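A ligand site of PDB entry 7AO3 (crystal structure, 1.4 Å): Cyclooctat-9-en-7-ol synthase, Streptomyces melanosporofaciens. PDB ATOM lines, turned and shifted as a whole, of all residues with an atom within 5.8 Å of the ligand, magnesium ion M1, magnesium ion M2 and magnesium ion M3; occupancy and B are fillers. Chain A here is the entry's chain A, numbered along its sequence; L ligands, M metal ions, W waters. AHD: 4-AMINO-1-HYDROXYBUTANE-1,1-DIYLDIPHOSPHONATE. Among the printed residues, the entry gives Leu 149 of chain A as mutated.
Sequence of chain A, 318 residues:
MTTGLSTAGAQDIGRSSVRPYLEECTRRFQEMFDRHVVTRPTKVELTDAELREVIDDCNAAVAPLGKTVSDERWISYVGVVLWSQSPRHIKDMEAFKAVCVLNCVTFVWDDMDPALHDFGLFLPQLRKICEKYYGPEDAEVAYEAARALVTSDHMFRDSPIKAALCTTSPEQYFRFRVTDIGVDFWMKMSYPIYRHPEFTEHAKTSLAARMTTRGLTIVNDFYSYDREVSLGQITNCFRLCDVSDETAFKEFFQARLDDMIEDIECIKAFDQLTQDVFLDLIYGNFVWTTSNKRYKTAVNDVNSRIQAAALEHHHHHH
O11 of the ligand lies within salt-bridge range of NH2 of Arg 227 (3.4 Å). The backbone carbonyl oxygen (O) of Ile 181 lies within hydrogen-bond range of a nitrogen (N4) of the ligand (3.3 Å). The guanidinium group (NH1) of Arg 177 is in salt-bridge range of an oxygen (O15) of the ligand, at 2.7 Å. NE of Arg 294 is in salt-bridge range of O11 of the ligand (2.7 Å). OH of Tyr 295 lies within hydrogen-bond range of O11 of the ligand (2.6 Å).
The side-chain amide nitrogen of Asn 236 sits at hydrogen-bond distance from the side-chain carboxylate of Glu 228, 2.9 Å away. The guanidinium group of Arg 294 lies within salt-bridge range of the side-chain carboxylate of Asp 111 (2.9 Å). The side-chain amide nitrogen (ND2) of Asn 220 is in hydrogen-bond range of the side-chain hydroxyl (OH) of Tyr 295 (3.3 Å). The backbone carbonyl oxygen (O) of Glu 228 lies within hydrogen-bond range of the backbone NH (N) of Gln 233, 2.9 Å away. NH2 of Arg 177 lies within salt-bridge range of OD1 of Asp 221 (2.9 Å). The guanidinium group (NH1) of Arg 177 is in salt-bridge range of the side-chain carboxylate (OD1) of Asp 180 (2.8 Å).
CE1 of Phe 107 touches C7 of the ligand (3.5 Å). Hydrophobic or aromatic side chains that line the ligand: Phe 107, Ile 181 and Tyr 295. Within 4 Å of the ligand: Phe 107, Asp 110, Arg 177, Ile 181, Asn 220, Ser 224, Arg 227, Glu 228, Arg 294 and Tyr 295.
Arg 177 touches magnesium ion M1 (NH2 to MG, 3.9 Å). Four residues have an atom within 4 Å of magnesium ion M1: Arg 177, Asn 220, Ser 224 and Glu 228. The nearest printed residue that does not touch magnesium ion M1 is Asp 221 (4.4 Å).
Merely in contact with magnesium ion M2: Arg 227 (3.97 Å). Two residues have an atom within 4 Å of magnesium ion M2: Asp 110 and Arg 227.
Of the 22 residues printed, 1 comes within 4 Å of magnesium ion M3. The nearest printed residue that does not touch magnesium ion M3 is Asp 180 (4.1 Å).
Magnesium ion M1 is bound by O16 of the ligand (2.0 Å), O10 of the ligand (2.1 Å), OE2 of Glu 228 (2.1 Å), OD1 of Asn 220 (2.1 Å), water W9 (2.1 Å) and OG of Ser 224 (2.3 Å).
The side-chain carboxylate (OD2) of Asp 110 binds magnesium ion M2 (2.0 Å). An oxygen (O12) of the ligand is bound to magnesium ion M2 (2.1 Å). An oxygen (O17) of the ligand binds magnesium ion M2 (2.1 Å). Magnesium ion M2 is bound by water W7. Water W3 binds magnesium ion M2. Water W11 binds magnesium ion M2, 2.4 Å away. Magnesium ion M2 has six donor atoms within binding distance.
Magnesium ion M3 is bound by water W11 (2.1 Å), O17 of the ligand (2.1 Å), OD1 of Asp 110 (2.1 Å), water W8 (2.1 Å), water W4 (2.1 Å) and water W2 (2.1 Å). Magnesium ion M3 has six donor atoms within binding distance.
Water W7 bridges OD1 of Asp 111 (2.9 Å) and NH1 of Arg 227 (3.5 Å). Water W4 bridges OD1 of Asp 180 and NH1 of Arg 177. Water W2 lies within hydrogen-bond range of O15 of the ligand and O of Asp 180. Water W1 lies within hydrogen-bond range of a nitrogen (N4) of the ligand (2.7 Å), the backbone carbonyl oxygen (O) of Ile 181 (3.2 Å) and the backbone carbonyl oxygen (O) of Asp 180 (3.3 Å). Water W5 lies within hydrogen-bond range of N4 of the ligand (2.7 Å), OG1 of Thr 106 (2.8 Å), O of Asn 103 (3.1 Å) and N of Phe 107 (3.4 Å). Water W10 lies within hydrogen-bond range of O13 of the ligand, OH of Tyr 295 and ND2 of Asn 220.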
ATOM      1  N   ASN A 103      26.361  10.984  -5.572  1.00  0.00           N
ATOM      2  CA  ASN A 103      25.198  10.475  -6.288  1.00  0.00           C
ATOM      3  C   ASN A 103      23.916  10.661  -5.474  1.00  0.00           C
ATOM      4  O   ASN A 103      22.848  10.871  -6.059  1.00  0.00           O
ATOM      5  CB  ASN A 103      25.442   9.047  -6.789  1.00  0.00           C
ATOM      6  CG  ASN A 103      24.657   8.704  -8.068  1.00  0.00           C
ATOM      7  OD1 ASN A 103      23.730   7.917  -8.041  1.00  0.00           O
ATOM      8  ND2 ASN A 103      25.056   9.287  -9.186  1.00  0.00           N
ATOM      9  N   THR A 106      22.999  14.655  -5.636  1.00  0.00           N
ATOM     10  CA  THR A 106      22.498  15.037  -6.957  1.00  0.00           C
ATOM     11  C   THR A 106      21.179  14.344  -7.291  1.00  0.00           C
ATOM     12  O   THR A 106      20.405  14.847  -8.112  1.00  0.00           O
ATOM     13  CB  THR A 106      23.562  14.848  -8.074  1.00  0.00           C
ATOM     14  OG1 THR A 106      23.989  13.477  -8.151  1.00  0.00           O
ATOM     15  CG2 THR A 106      24.757  15.727  -7.797  1.00  0.00           C
ATOM     16  N   PHE A 107      20.869  13.211  -6.636  1.00  0.00           N
ATOM     17  CA  PHE A 107      19.534  12.643  -6.775  1.00  0.00           C
ATOM     18  C   PHE A 107      18.488  13.564  -6.178  1.00  0.00           C
ATOM     19  O   PHE A 107      17.380  13.711  -6.731  1.00  0.00           O
ATOM     20  CB  PHE A 107      19.475  11.299  -6.038  1.00  0.00           C
ATOM     21  CG  PHE A 107      19.147  10.136  -6.918  1.00  0.00           C
ATOM     22  CD1 PHE A 107      17.916  10.070  -7.581  1.00  0.00           C
ATOM     23  CD2 PHE A 107      20.013   9.060  -7.020  1.00  0.00           C
ATOM     24  CE1 PHE A 107      17.596   9.030  -8.341  1.00  0.00           C
ATOM     25  CE2 PHE A 107      19.644   7.954  -7.798  1.00  0.00           C
ATOM     26  CZ  PHE A 107      18.418   7.960  -8.448  1.00  0.00           C
ATOM     27  N   ASP A 110      17.818  16.245  -8.645  1.00  0.00           N
ATOM     28  CA  ASP A 110      16.969  15.680  -9.700  1.00  0.00           C
ATOM     29  C   ASP A 110      15.506  15.657  -9.278  1.00  0.00           C
ATOM     30  O   ASP A 110      14.609  15.905 -10.099  1.00  0.00           O
ATOM     31  CB  ASP A 110      17.443  14.238  -9.992  1.00  0.00           C
ATOM     32  CG  ASP A 110      16.816  13.636 -11.242  1.00  0.00           C
ATOM     33  OD1 ASP A 110      17.225  14.015 -12.375  1.00  0.00           O
ATOM     34  OD2 ASP A 110      15.888  12.784 -11.088  1.00  0.00           O
ATOM     35  N   ASP A 111      15.250  15.329  -8.004  1.00  0.00           N
ATOM     36  CA  ASP A 111      13.884  15.211  -7.495  1.00  0.00           C
ATOM     37  C   ASP A 111      13.263  16.545  -7.099  1.00  0.00           C
ATOM     38  O   ASP A 111      12.072  16.565  -6.785  1.00  0.00           O
ATOM     39  CB  ASP A 111      13.826  14.238  -6.299  1.00  0.00           C
ATOM     40  CG  ASP A 111      13.773  12.786  -6.711  1.00  0.00           C
ATOM     41  OD1 ASP A 111      13.412  12.468  -7.885  1.00  0.00           O
ATOM     42  OD2 ASP A 111      14.061  11.958  -5.844  1.00  0.00           O
ATOM     43  N   LEU A 149      26.522  18.439 -14.356  1.00  0.00           N
ATOM     44  CA  LEU A 149      25.271  17.683 -14.263  1.00  0.00           C
ATOM     45  C   LEU A 149      24.152  18.521 -13.647  1.00  0.00           C
ATOM     46  O   LEU A 149      23.045  18.615 -14.211  1.00  0.00           O
ATOM     47  CB  LEU A 149      25.502  16.384 -13.487  1.00  0.00           C
ATOM     48  CG  LEU A 149      24.179  15.619 -13.262  1.00  0.00           C
ATOM     49  CD1 LEU A 149      23.488  15.195 -14.581  1.00  0.00           C
ATOM     50  CD2 LEU A 149      24.452  14.443 -12.367  1.00  0.00           C
ATOM     51  N   ASP A 153      20.733  19.583 -15.473  1.00  0.00           N
ATOM     52  CA  ASP A 153      19.385  19.270 -14.991  1.00  0.00           C
ATOM     53  C   ASP A 153      18.532  20.520 -14.877  1.00  0.00           C
ATOM     54  O   ASP A 153      17.361  20.538 -15.295  1.00  0.00           O
ATOM     55  CB  ASP A 153      19.456  18.567 -13.631  1.00  0.00           C
ATOM     56  CG  ASP A 153      18.114  18.348 -13.045  1.00  0.00           C
ATOM     57  OD1 ASP A 153      17.324  17.544 -13.567  1.00  0.00           O
ATOM     58  OD2 ASP A 153      17.820  19.072 -12.094  1.00  0.00           O
ATOM     59  N   ARG A 177      20.972  11.817 -23.138  1.00  0.00           N
ATOM     60  CA  ARG A 177      21.076  11.110 -21.855  1.00  0.00           C
ATOM     61  C   ARG A 177      22.513  10.805 -21.398  1.00  0.00           C
ATOM     62  O   ARG A 177      22.724  10.556 -20.195  1.00  0.00           O
ATOM     63  CB  ARG A 177      20.271   9.799 -21.907  1.00  0.00           C
ATOM     64  CG  ARG A 177      18.773  10.075 -21.949  1.00  0.00           C
ATOM     65  CD  ARG A 177      18.282  10.661 -20.613  1.00  0.00           C
ATOM     66  NE  ARG A 177      17.416   9.705 -19.909  1.00  0.00           N
ATOM     67  CZ  ARG A 177      17.244   9.671 -18.569  1.00  0.00           C
ATOM     68  NH1 ARG A 177      17.845  10.558 -17.778  1.00  0.00           N
ATOM     69  NH2 ARG A 177      16.507   8.713 -17.986  1.00  0.00           N
ATOM     70  N   ASP A 180      22.528  13.639 -19.282  1.00  0.00           N
ATOM     71  CA  ASP A 180      21.351  13.871 -18.440  1.00  0.00           C
ATOM     72  C   ASP A 180      21.117  12.781 -17.391  1.00  0.00           C
ATOM     73  O   ASP A 180      20.662  13.089 -16.279  1.00  0.00           O
ATOM     74  CB  ASP A 180      20.104  14.043 -19.317  1.00  0.00           C
ATOM     75  CG  ASP A 180      18.830  14.266 -18.486  1.00  0.00           C
ATOM     76  OD1 ASP A 180      18.118  13.283 -18.177  1.00  0.00           O
ATOM     77  OD2 ASP A 180      18.474  15.426 -18.220  1.00  0.00           O
ATOM     78  N   ILE A 181      21.360  11.508 -17.739  1.00  0.00           N
ATOM     79  CA  ILE A 181      21.128  10.446 -16.760  1.00  0.00           C
ATOM     80  C   ILE A 181      22.175  10.492 -15.659  1.00  0.00           C
ATOM     81  O   ILE A 181      21.964   9.883 -14.612  1.00  0.00           O
ATOM     82  CB  ILE A 181      20.979   9.048 -17.387  1.00  0.00           C
ATOM     83  CG1 ILE A 181      20.219   8.116 -16.422  1.00  0.00           C
ATOM     84  CG2 ILE A 181      22.363   8.417 -17.791  1.00  0.00           C
ATOM     85  CD1 ILE A 181      19.740   6.843 -17.067  1.00  0.00           C
ATOM     86  N   GLY A 182      23.280  11.224 -15.868  1.00  0.00           N
ATOM     87  CA  GLY A 182      24.310  11.329 -14.877  1.00  0.00           C
ATOM     88  C   GLY A 182      25.466  10.352 -15.060  1.00  0.00           C
ATOM     89  O   GLY A 182      26.327  10.271 -14.179  1.00  0.00           O
ATOM     90  N   ASN A 220      16.323   2.177 -16.792  1.00  0.00           N
ATOM     91  CA  ASN A 220      15.731   3.193 -15.934  1.00  0.00           C
ATOM     92  C   ASN A 220      14.425   3.707 -16.500  1.00  0.00           C
ATOM     93  O   ASN A 220      13.450   3.932 -15.763  1.00  0.00           O
ATOM     94  CB  ASN A 220      16.667   4.393 -15.756  1.00  0.00           C
ATOM     95  CG  ASN A 220      15.993   5.486 -14.961  1.00  0.00           C
ATOM     96  OD1 ASN A 220      15.409   6.441 -15.524  1.00  0.00           O
ATOM     97  ND2 ASN A 220      15.959   5.300 -13.637  1.00  0.00           N
ATOM     98  N   ASP A 221      14.402   3.922 -17.819  1.00  0.00           N
ATOM     99  CA  ASP A 221      13.229   4.513 -18.448  1.00  0.00           C
ATOM    100  C   ASP A 221      12.018   3.581 -18.320  1.00  0.00           C
ATOM    101  O   ASP A 221      10.886   4.041 -18.051  1.00  0.00           O
ATOM    102  CB  ASP A 221      13.492   4.784 -19.932  1.00  0.00           C
ATOM    103  CG  ASP A 221      14.386   5.986 -20.183  1.00  0.00           C
ATOM    104  OD1 ASP A 221      14.777   6.685 -19.218  1.00  0.00           O
ATOM    105  OD2 ASP A 221      14.657   6.239 -21.392  1.00  0.00           O
ATOM    106  N   SER A 224      10.876   3.803 -14.552  1.00  0.00           N
ATOM    107  CA  SER A 224      10.523   5.122 -14.069  1.00  0.00           C
ATOM    108  C   SER A 224       9.493   5.825 -14.952  1.00  0.00           C
ATOM    109  O   SER A 224       9.080   6.935 -14.623  1.00  0.00           O
ATOM    110  CB  SER A 224      11.762   6.002 -13.851  1.00  0.00           C
ATOM    111  OG  SER A 224      12.481   6.301 -15.045  1.00  0.00           O
ATOM    112  N   ARG A 227       6.109   7.057 -13.034  1.00  0.00           N
ATOM    113  CA  ARG A 227       6.355   8.246 -12.238  1.00  0.00           C
ATOM    114  C   ARG A 227       6.536   9.467 -13.132  1.00  0.00           C
ATOM    115  O   ARG A 227       5.922  10.519 -12.918  1.00  0.00           O
ATOM    116  CB  ARG A 227       7.601   8.043 -11.368  1.00  0.00           C
ATOM    117  CG  ARG A 227       8.161   9.349 -10.819  1.00  0.00           C
ATOM    118  CD  ARG A 227       9.145   9.158  -9.670  1.00  0.00           C
ATOM    119  NE  ARG A 227      10.125   8.122  -9.934  1.00  0.00           N
ATOM    120  CZ  ARG A 227      11.285   8.312 -10.560  1.00  0.00           C
ATOM    121  NH1 ARG A 227      11.630   9.541 -11.012  1.00  0.00           N
ATOM    122  NH2 ARG A 227      12.090   7.264 -10.722  1.00  0.00           N
ATOM    123  N   GLU A 228       7.380   9.337 -14.170  1.00  0.00           N
ATOM    124  CA  GLU A 228       7.758  10.484 -14.997  1.00  0.00           C
ATOM    125  C   GLU A 228       6.564  11.021 -15.771  1.00  0.00           C
ATOM    126  O   GLU A 228       6.318  12.233 -15.793  1.00  0.00           O
ATOM    127  CB  GLU A 228       8.948  10.103 -15.886  1.00  0.00           C
ATOM    128  CG  GLU A 228      10.173   9.991 -15.000  1.00  0.00           C
ATOM    129  CD  GLU A 228      11.377   9.383 -15.661  1.00  0.00           C
ATOM    130  OE1 GLU A 228      11.301   9.032 -16.856  1.00  0.00           O
ATOM    131  OE2 GLU A 228      12.390   9.222 -14.949  1.00  0.00           O
ATOM    132  N   GLN A 233       7.265  14.739 -16.897  1.00  0.00           N
ATOM    133  CA  GLN A 233       8.670  14.684 -17.294  1.00  0.00           C
ATOM    134  C   GLN A 233       8.778  13.920 -18.609  1.00  0.00           C
ATOM    135  O   GLN A 233       8.301  12.788 -18.706  1.00  0.00           O
ATOM    136  CB  GLN A 233       9.451  13.961 -16.187  1.00  0.00           C
ATOM    137  CG  GLN A 233       9.621  14.882 -14.968  1.00  0.00           C
ATOM    138  CD  GLN A 233      10.122  14.169 -13.729  1.00  0.00           C
ATOM    139  OE1 GLN A 233       9.659  13.065 -13.382  1.00  0.00           O
ATOM    140  NE2 GLN A 233      11.088  14.793 -13.059  1.00  0.00           N
ATOM    141  N   THR A 235      11.666  13.094 -20.309  1.00  0.00           N
ATOM    142  CA  THR A 235      12.972  12.470 -20.609  1.00  0.00           C
ATOM    143  C   THR A 235      12.819  10.962 -20.382  1.00  0.00           C
ATOM    144  O   THR A 235      13.194  10.407 -19.346  1.00  0.00           O
ATOM    145  CB  THR A 235      14.078  13.093 -19.762  1.00  0.00           C
ATOM    146  OG1 THR A 235      14.058  14.509 -19.959  1.00  0.00           O
ATOM    147  CG2 THR A 235      15.473  12.610 -20.193  1.00  0.00           C
ATOM    148  N   ASN A 236      12.259  10.272 -21.382  1.00  0.00           N
ATOM    149  CA  ASN A 236      12.014   8.838 -21.268  1.00  0.00           C
ATOM    150  C   ASN A 236      11.830   8.278 -22.675  1.00  0.00           C
ATOM    151  O   ASN A 236      10.952   8.735 -23.415  1.00  0.00           O
ATOM    152  CB  ASN A 236      10.740   8.601 -20.396  1.00  0.00           C
ATOM    153  CG  ASN A 236      10.615   7.162 -19.990  1.00  0.00           C
ATOM    154  OD1 ASN A 236      10.522   6.288 -20.869  1.00  0.00           O
ATOM    155  ND2 ASN A 236      10.657   6.876 -18.682  1.00  0.00           N
ATOM    156  N   TRP A 288      19.280  -3.083  -8.675  1.00  0.00           N
ATOM    157  CA  TRP A 288      18.771  -2.071  -7.749  1.00  0.00           C
ATOM    158  C   TRP A 288      17.429  -1.523  -8.209  1.00  0.00           C
ATOM    159  O   TRP A 288      16.491  -1.380  -7.406  1.00  0.00           O
ATOM    160  CB  TRP A 288      19.812  -0.942  -7.646  1.00  0.00           C
ATOM    161  CG  TRP A 288      19.310   0.303  -6.954  1.00  0.00           C
ATOM    162  CD1 TRP A 288      19.079   0.480  -5.613  1.00  0.00           C
ATOM    163  CD2 TRP A 288      18.990   1.544  -7.581  1.00  0.00           C
ATOM    164  NE1 TRP A 288      18.641   1.766  -5.367  1.00  0.00           N
ATOM    165  CE2 TRP A 288      18.596   2.446  -6.568  1.00  0.00           C
ATOM    166  CE3 TRP A 288      19.017   1.978  -8.914  1.00  0.00           C
ATOM    167  CZ2 TRP A 288      18.233   3.764  -6.839  1.00  0.00           C
ATOM    168  CZ3 TRP A 288      18.648   3.289  -9.195  1.00  0.00           C
ATOM    169  CH2 TRP A 288      18.263   4.173  -8.146  1.00  0.00           C
ATOM    170  N   ARG A 294      12.066   2.950  -4.804  1.00  0.00           N
ATOM    171  CA  ARG A 294      11.957   4.121  -5.683  1.00  0.00           C
ATOM    172  C   ARG A 294      11.164   3.812  -6.952  1.00  0.00           C
ATOM    173  O   ARG A 294      10.498   4.687  -7.492  1.00  0.00           O
ATOM    174  CB  ARG A 294      13.368   4.614  -6.062  1.00  0.00           C
ATOM    175  CG  ARG A 294      13.343   5.743  -7.140  1.00  0.00           C
ATOM    176  CD  ARG A 294      14.697   6.420  -7.331  1.00  0.00           C
ATOM    177  NE  ARG A 294      14.640   7.604  -8.203  1.00  0.00           N
ATOM    178  CZ  ARG A 294      14.240   8.809  -7.804  1.00  0.00           C
ATOM    179  NH1 ARG A 294      13.880   8.984  -6.526  1.00  0.00           N
ATOM    180  NH2 ARG A 294      14.197   9.819  -8.675  1.00  0.00           N
ATOM    181  N   TYR A 295      11.261   2.584  -7.466  1.00  0.00           N
ATOM    182  CA  TYR A 295      10.610   2.192  -8.716  1.00  0.00           C
ATOM    183  C   TYR A 295       9.422   1.254  -8.500  1.00  0.00           C
ATOM    184  O   TYR A 295       8.869   0.728  -9.467  1.00  0.00           O
ATOM    185  CB  TYR A 295      11.648   1.564  -9.680  1.00  0.00           C
ATOM    186  CG  TYR A 295      12.823   2.495  -9.893  1.00  0.00           C
ATOM    187  CD1 TYR A 295      12.724   3.588 -10.770  1.00  0.00           C
ATOM    188  CD2 TYR A 295      14.000   2.341  -9.172  1.00  0.00           C
ATOM    189  CE1 TYR A 295      13.813   4.514 -10.943  1.00  0.00           C
ATOM    190  CE2 TYR A 295      15.084   3.214  -9.344  1.00  0.00           C
ATOM    191  CZ  TYR A 295      14.982   4.309 -10.230  1.00  0.00           C
ATOM    192  OH  TYR A 295      15.996   5.216 -10.381  1.00  0.00           O
HETATM  193  C2  AHD L   1      19.063  10.019 -12.191  1.00  0.00           C
HETATM  194  C3  AHD L   1      19.935  10.319 -10.994  1.00  0.00           C
HETATM  195  C7  AHD L   1      17.645   9.705 -11.771  1.00  0.00           C
HETATM  196  C8  AHD L   1      16.778   9.020 -12.835  1.00  0.00           C
HETATM  197  O12 AHD L   1      14.522   9.886 -11.619  1.00  0.00           O
HETATM  198  P9  AHD L   1      15.144   8.576 -12.054  1.00  0.00           P
HETATM  199  O10 AHD L   1      14.296   7.791 -13.027  1.00  0.00           O
HETATM  200  O11 AHD L   1      15.419   7.730 -10.828  1.00  0.00           O
HETATM  201  P14 AHD L   1      16.452  10.088 -14.319  1.00  0.00           P
HETATM  202  O15 AHD L   1      17.803  10.235 -15.076  1.00  0.00           O
HETATM  203  O16 AHD L   1      15.349   9.487 -15.174  1.00  0.00           O
HETATM  204  O17 AHD L   1      16.034  11.477 -13.777  1.00  0.00           O
HETATM  205  O13 AHD L   1      17.368   7.833 -13.329  1.00  0.00           O
HETATM  206  N4  AHD L   1      21.353  10.473 -11.405  1.00  0.00           N
HETATM  207 MG    MG M   1      14.034   7.944 -15.065  1.00  0.00          MG
HETATM  208 MG    MG M   2      14.590  11.857 -12.280  1.00  0.00          MG
HETATM  209 MG    MG M   3      16.648  13.396 -14.305  1.00  0.00          MG
HETATM  210  O   HOH W   1      21.428  12.601 -13.084  1.00  0.00           O
HETATM  211  O   HOH W   2      18.598  12.592 -14.600  1.00  0.00           O
HETATM  212  O   HOH W   3      12.906  11.382 -13.488  1.00  0.00           O
HETATM  213  O   HOH W   4      16.152  13.089 -16.349  1.00  0.00           O
HETATM  214  O   HOH W   5      22.431  11.336  -9.047  1.00  0.00           O
HETATM  215  O   HOH W   6      14.255  11.227 -16.807  1.00  0.00           O
HETATM  216  O   HOH W   7      13.246  12.619 -10.823  1.00  0.00           O
HETATM  217  O   HOH W   8      17.208  15.334 -14.951  1.00  0.00           O
HETATM  218  O   HOH W   9      13.725   7.992 -17.163  1.00  0.00           O
HETATM  219  O   HOH W  10      18.513   6.056 -11.495  1.00  0.00           O
HETATM  220  O   HOH W  11      14.714  13.791 -13.671  1.00  0.00           O
